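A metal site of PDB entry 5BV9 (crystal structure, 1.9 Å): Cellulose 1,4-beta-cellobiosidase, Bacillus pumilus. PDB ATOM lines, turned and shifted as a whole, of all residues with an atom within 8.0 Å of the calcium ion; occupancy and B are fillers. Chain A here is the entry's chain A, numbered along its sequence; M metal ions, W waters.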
ATOM      1  N   PRO A 112      15.459 -13.513 -31.474  1.00  0.00           N
ATOM      2  CA  PRO A 112      14.228 -13.050 -32.132  1.00  0.00           C
ATOM      3  C   PRO A 112      13.021 -14.013 -32.023  1.00  0.00           C
ATOM      4  O   PRO A 112      11.880 -13.568 -32.300  1.00  0.00           O
ATOM      5  CB  PRO A 112      14.627 -12.909 -33.585  1.00  0.00           C
ATOM      6  CG  PRO A 112      15.836 -13.766 -33.765  1.00  0.00           C
ATOM      7  CD  PRO A 112      16.503 -13.893 -32.436  1.00  0.00           C
ATOM      8  N   TYR A 113      13.287 -15.281 -31.693  1.00  0.00           N
ATOM      9  CA  TYR A 113      12.221 -16.275 -31.394  1.00  0.00           C
ATOM     10  C   TYR A 113      12.527 -17.101 -30.177  1.00  0.00           C
ATOM     11  O   TYR A 113      13.681 -17.365 -29.943  1.00  0.00           O
ATOM     12  CB  TYR A 113      12.055 -17.293 -32.548  1.00  0.00           C
ATOM     13  CG  TYR A 113      11.634 -16.559 -33.800  1.00  0.00           C
ATOM     14  CD1 TYR A 113      10.325 -16.141 -33.986  1.00  0.00           C
ATOM     15  CD2 TYR A 113      12.588 -16.223 -34.768  1.00  0.00           C
ATOM     16  CE1 TYR A 113       9.963 -15.373 -35.106  1.00  0.00           C
ATOM     17  CE2 TYR A 113      12.219 -15.539 -35.931  1.00  0.00           C
ATOM     18  CZ  TYR A 113      10.907 -15.123 -36.087  1.00  0.00           C
ATOM     19  OH  TYR A 113      10.619 -14.401 -37.238  1.00  0.00           O
ATOM     20  N   PRO A 114      11.504 -17.511 -29.413  1.00  0.00           N
ATOM     21  CA  PRO A 114      11.754 -18.411 -28.315  1.00  0.00           C
ATOM     22  C   PRO A 114      12.484 -19.692 -28.679  1.00  0.00           C
ATOM     23  O   PRO A 114      13.224 -20.214 -27.848  1.00  0.00           O
ATOM     24  CB  PRO A 114      10.378 -18.761 -27.830  1.00  0.00           C
ATOM     25  CG  PRO A 114       9.451 -17.716 -28.370  1.00  0.00           C
ATOM     26  CD  PRO A 114      10.062 -17.327 -29.656  1.00  0.00           C
ATOM     27  N   ASP A 115      12.285 -20.147 -29.930  1.00  0.00           N
ATOM     28  CA  ASP A 115      12.958 -21.298 -30.493  1.00  0.00           C
ATOM     29  C   ASP A 115      14.451 -21.289 -30.403  1.00  0.00           C
ATOM     30  O   ASP A 115      15.056 -22.336 -30.432  1.00  0.00           O
ATOM     31  CB  ASP A 115      12.591 -21.482 -31.989  1.00  0.00           C
ATOM     32  CG  ASP A 115      11.103 -21.337 -32.273  1.00  0.00           C
ATOM     33  OD1 ASP A 115      10.508 -20.284 -31.826  1.00  0.00           O
ATOM     34  OD2 ASP A 115      10.588 -22.197 -32.990  1.00  0.00           O
ATOM     35  N   GLY A 179      12.574 -13.487 -25.114  1.00  0.00           N
ATOM     36  CA  GLY A 179      12.655 -12.495 -26.182  1.00  0.00           C
ATOM     37  C   GLY A 179      11.339 -11.976 -26.664  1.00  0.00           C
ATOM     38  O   GLY A 179      10.228 -12.295 -26.122  1.00  0.00           O
ATOM     39  N   GLN A 180      11.433 -11.225 -27.762  1.00  0.00           N
ATOM     40  CA  GLN A 180      10.375 -10.403 -28.247  1.00  0.00           C
ATOM     41  C   GLN A 180       9.196 -11.142 -28.796  1.00  0.00           C
ATOM     42  O   GLN A 180       8.087 -10.559 -28.842  1.00  0.00           O
ATOM     43  CB  GLN A 180      10.913  -9.420 -29.300  1.00  0.00           C
ATOM     44  CG  GLN A 180      11.341 -10.062 -30.614  1.00  0.00           C
ATOM     45  CD  GLN A 180      12.261  -9.132 -31.407  1.00  0.00           C
ATOM     46  OE1 GLN A 180      12.698  -8.125 -30.903  1.00  0.00           O
ATOM     47  NE2 GLN A 180      12.510  -9.459 -32.632  1.00  0.00           N
ATOM     48  N   GLN A 181       9.431 -12.354 -29.265  1.00  0.00           N
ATOM     49  CA  GLN A 181       8.331 -13.159 -29.806  1.00  0.00           C
ATOM     50  C   GLN A 181       7.679 -14.104 -28.817  1.00  0.00           C
ATOM     51  O   GLN A 181       6.804 -14.899 -29.186  1.00  0.00           O
ATOM     52  CB  GLN A 181       8.778 -13.905 -31.055  1.00  0.00           C
ATOM     53  CG  GLN A 181       8.524 -13.178 -32.361  1.00  0.00           C
ATOM     54  CD  GLN A 181       7.016 -12.955 -32.611  1.00  0.00           C
ATOM     55  OE1 GLN A 181       6.180 -13.710 -32.187  1.00  0.00           O
ATOM     56  NE2 GLN A 181       6.711 -11.910 -33.333  1.00  0.00           N
ATOM     57  N   GLU A 182       8.063 -14.075 -27.551  1.00  0.00           N
ATOM     58  CA  GLU A 182       7.400 -14.965 -26.624  1.00  0.00           C
ATOM     59  C   GLU A 182       6.154 -14.264 -26.125  1.00  0.00           C
ATOM     60  O   GLU A 182       6.246 -13.453 -25.197  1.00  0.00           O
ATOM     61  CB  GLU A 182       8.325 -15.258 -25.426  1.00  0.00           C
ATOM     62  CG  GLU A 182       7.765 -16.351 -24.484  1.00  0.00           C
ATOM     63  CD  GLU A 182       8.674 -16.669 -23.353  1.00  0.00           C
ATOM     64  OE1 GLU A 182       9.186 -15.717 -22.713  1.00  0.00           O
ATOM     65  OE2 GLU A 182       8.883 -17.846 -23.141  1.00  0.00           O
ATOM     66  N   SER A 183       5.014 -14.513 -26.741  1.00  0.00           N
ATOM     67  CA  SER A 183       3.759 -13.961 -26.223  1.00  0.00           C
ATOM     68  C   SER A 183       3.418 -14.576 -24.883  1.00  0.00           C
ATOM     69  O   SER A 183       4.004 -15.588 -24.475  1.00  0.00           O
ATOM     70  CB  SER A 183       2.589 -14.201 -27.191  1.00  0.00           C
ATOM     71  OG  SER A 183       2.195 -15.591 -27.185  1.00  0.00           O
ATOM     72  N   VAL A 184       2.364 -14.059 -24.269  1.00  0.00           N
ATOM     73  CA  VAL A 184       1.861 -14.624 -23.017  1.00  0.00           C
ATOM     74  C   VAL A 184       1.495 -16.124 -23.214  1.00  0.00           C
ATOM     75  O   VAL A 184       1.732 -17.011 -22.331  1.00  0.00           O
ATOM     76  CB  VAL A 184       0.672 -13.816 -22.438  1.00  0.00           C
ATOM     77  CG1 VAL A 184      -0.536 -13.811 -23.390  1.00  0.00           C
ATOM     78  CG2 VAL A 184       0.242 -14.392 -21.108  1.00  0.00           C
ATOM     79  N   TRP A 185       1.053 -16.441 -24.401  1.00  0.00           N
ATOM     80  CA  TRP A 185       0.660 -17.826 -24.748  1.00  0.00           C
ATOM     81  C   TRP A 185       1.831 -18.775 -24.921  1.00  0.00           C
ATOM     82  O   TRP A 185       1.661 -19.994 -24.927  1.00  0.00           O
ATOM     83  CB  TRP A 185      -0.106 -17.798 -26.088  1.00  0.00           C
ATOM     84  CG  TRP A 185      -1.203 -16.858 -26.065  1.00  0.00           C
ATOM     85  CD1 TRP A 185      -1.248 -15.590 -26.613  1.00  0.00           C
ATOM     86  CD2 TRP A 185      -2.461 -17.072 -25.471  1.00  0.00           C
ATOM     87  NE1 TRP A 185      -2.490 -15.021 -26.381  1.00  0.00           N
ATOM     88  CE2 TRP A 185      -3.237 -15.907 -25.640  1.00  0.00           C
ATOM     89  CE3 TRP A 185      -3.033 -18.169 -24.799  1.00  0.00           C
ATOM     90  CZ2 TRP A 185      -4.539 -15.832 -25.220  1.00  0.00           C
ATOM     91  CZ3 TRP A 185      -4.272 -18.035 -24.295  1.00  0.00           C
ATOM     92  CH2 TRP A 185      -5.027 -16.886 -24.530  1.00  0.00           C
ATOM     93  N   GLU A 186       3.001 -18.217 -25.132  1.00  0.00           N
ATOM     94  CA  GLU A 186       4.217 -18.998 -25.491  1.00  0.00           C
ATOM     95  C   GLU A 186       5.208 -19.173 -24.345  1.00  0.00           C
ATOM     96  O   GLU A 186       6.274 -19.822 -24.537  1.00  0.00           O
ATOM     97  CB  GLU A 186       4.849 -18.319 -26.678  1.00  0.00           C
ATOM     98  CG  GLU A 186       4.001 -18.405 -27.947  1.00  0.00           C
ATOM     99  CD  GLU A 186       4.518 -17.447 -28.970  1.00  0.00           C
ATOM    100  OE1 GLU A 186       5.370 -17.815 -29.777  1.00  0.00           O
ATOM    101  OE2 GLU A 186       4.128 -16.289 -28.917  1.00  0.00           O
ATOM    102  N   HIS A 404       6.671  -8.064 -29.276  1.00  0.00           N
ATOM    103  CA  HIS A 404       6.155  -7.952 -30.590  1.00  0.00           C
ATOM    104  C   HIS A 404       4.925  -8.802 -30.846  1.00  0.00           C
ATOM    105  O   HIS A 404       4.341  -8.690 -31.939  1.00  0.00           O
ATOM    106  CB  HIS A 404       7.227  -8.422 -31.582  1.00  0.00           C
ATOM    107  CG  HIS A 404       8.380  -7.493 -31.692  1.00  0.00           C
ATOM    108  ND1 HIS A 404       9.374  -7.658 -32.612  1.00  0.00           N
ATOM    109  CD2 HIS A 404       8.707  -6.394 -30.985  1.00  0.00           C
ATOM    110  CE1 HIS A 404      10.244  -6.684 -32.504  1.00  0.00           C
ATOM    111  NE2 HIS A 404       9.856  -5.901 -31.511  1.00  0.00           N
ATOM    112  N   ASP A 405       4.482  -9.572 -29.850  1.00  0.00           N
ATOM    113  CA  ASP A 405       3.342 -10.479 -30.069  1.00  0.00           C
ATOM    114  C   ASP A 405       2.352 -10.331 -28.925  1.00  0.00           C
ATOM    115  O   ASP A 405       2.436 -11.072 -27.938  1.00  0.00           O
ATOM    116  CB  ASP A 405       3.910 -11.905 -30.232  1.00  0.00           C
ATOM    117  CG  ASP A 405       2.886 -12.926 -30.682  1.00  0.00           C
ATOM    118  OD1 ASP A 405       1.688 -12.606 -30.866  1.00  0.00           O
ATOM    119  OD2 ASP A 405       3.316 -14.094 -30.775  1.00  0.00           O
ATOM    120  N   PRO A 406       1.426  -9.367 -28.980  1.00  0.00           N
ATOM    121  CA  PRO A 406       1.235  -8.387 -30.033  1.00  0.00           C
ATOM    122  C   PRO A 406       2.268  -7.195 -29.819  1.00  0.00           C
ATOM    123  O   PRO A 406       2.828  -7.031 -28.700  1.00  0.00           O
ATOM    124  CB  PRO A 406      -0.178  -7.904 -29.772  1.00  0.00           C
ATOM    125  CG  PRO A 406      -0.333  -7.961 -28.277  1.00  0.00           C
ATOM    126  CD  PRO A 406       0.504  -9.130 -27.843  1.00  0.00           C
ATOM    127  N   ARG A 597      -5.439 -19.317 -29.129  1.00  0.00           N
ATOM    128  CA  ARG A 597      -4.062 -19.618 -28.635  1.00  0.00           C
ATOM    129  C   ARG A 597      -3.968 -20.419 -27.315  1.00  0.00           C
ATOM    130  O   ARG A 597      -2.884 -20.838 -26.881  1.00  0.00           O
ATOM    131  CB  ARG A 597      -3.284 -18.306 -28.578  1.00  0.00           C
ATOM    132  CG  ARG A 597      -3.279 -17.624 -29.956  1.00  0.00           C
ATOM    133  CD  ARG A 597      -2.419 -16.376 -29.922  1.00  0.00           C
ATOM    134  NE  ARG A 597      -0.975 -16.698 -30.021  1.00  0.00           N
ATOM    135  CZ  ARG A 597       0.013 -15.819 -30.118  1.00  0.00           C
ATOM    136  NH1 ARG A 597       1.291 -16.244 -30.192  1.00  0.00           N
ATOM    137  NH2 ARG A 597      -0.248 -14.518 -30.193  1.00  0.00           N
ATOM    138  N   GLU A 602       2.225 -23.963 -30.042  1.00  0.00           N
ATOM    139  CA  GLU A 602       3.205 -22.925 -30.197  1.00  0.00           C
ATOM    140  C   GLU A 602       4.008 -22.656 -28.944  1.00  0.00           C
ATOM    141  O   GLU A 602       4.755 -21.691 -28.913  1.00  0.00           O
ATOM    142  CB  GLU A 602       2.548 -21.609 -30.696  1.00  0.00           C
ATOM    143  CG  GLU A 602       3.520 -20.804 -31.546  1.00  0.00           C
ATOM    144  CD  GLU A 602       2.918 -19.563 -32.152  1.00  0.00           C
ATOM    145  OE1 GLU A 602       3.513 -19.072 -33.144  1.00  0.00           O
ATOM    146  OE2 GLU A 602       1.879 -19.107 -31.648  1.00  0.00           O
ATOM    147  N   ARG A 631      12.282 -20.356 -37.601  1.00  0.00           N
ATOM    148  CA  ARG A 631      12.553 -19.622 -36.374  1.00  0.00           C
ATOM    149  C   ARG A 631      13.819 -19.990 -35.736  1.00  0.00           C
ATOM    150  O   ARG A 631      14.112 -19.513 -34.641  1.00  0.00           O
ATOM    151  CB  ARG A 631      11.430 -19.809 -35.401  1.00  0.00           C
ATOM    152  CG  ARG A 631      10.122 -19.387 -36.057  1.00  0.00           C
ATOM    153  CD  ARG A 631       8.959 -19.350 -35.094  1.00  0.00           C
ATOM    154  NE  ARG A 631       7.756 -19.038 -35.830  1.00  0.00           N
ATOM    155  CZ  ARG A 631       6.518 -19.111 -35.362  1.00  0.00           C
ATOM    156  NH1 ARG A 631       6.276 -19.465 -34.115  1.00  0.00           N
ATOM    157  NH2 ARG A 631       5.505 -18.799 -36.155  1.00  0.00           N
HETATM  158 CA    CA M   1       5.242 -15.427 -30.921  1.00  0.00          CA
HETATM  159  O   HOH W   1       7.202 -16.788 -31.998  1.00  0.00           O
HETATM  160  O   HOH W   2       4.029 -16.413 -32.595  1.00  0.00           O
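The calcium ion is bound by water W2 (2.3 Å), the side-chain amide oxygen (OE1) of Gln 181 (2.3 Å), the side-chain carboxylate (OD2) of Asp 405 (2.3 Å), the backbone carbonyl oxygen (O) of Gln 181 (2.4 Å), the side-chain carboxylate (OE2) of Glu 186 (2.4 Å), water W1 (2.6 Å) and the side-chain carboxylate (OE1) of Glu 186 (2.7 Å).
The backbone NH of Glu 186 sits close to the side-chain hydroxyl of Ser 183, at 3.4 Å. NH1 of Arg 597 sits close to OE2 of Glu 186 (3.1 Å). The guanidinium group (NH2) of Arg 597 lies within salt-bridge range of the side-chain carboxylate (OD1) of Asp 405, 2.8 Å away.
Three residues have an atom within 4 Å of the calcium ion: Gln 181, Glu 186 and Asp 405.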
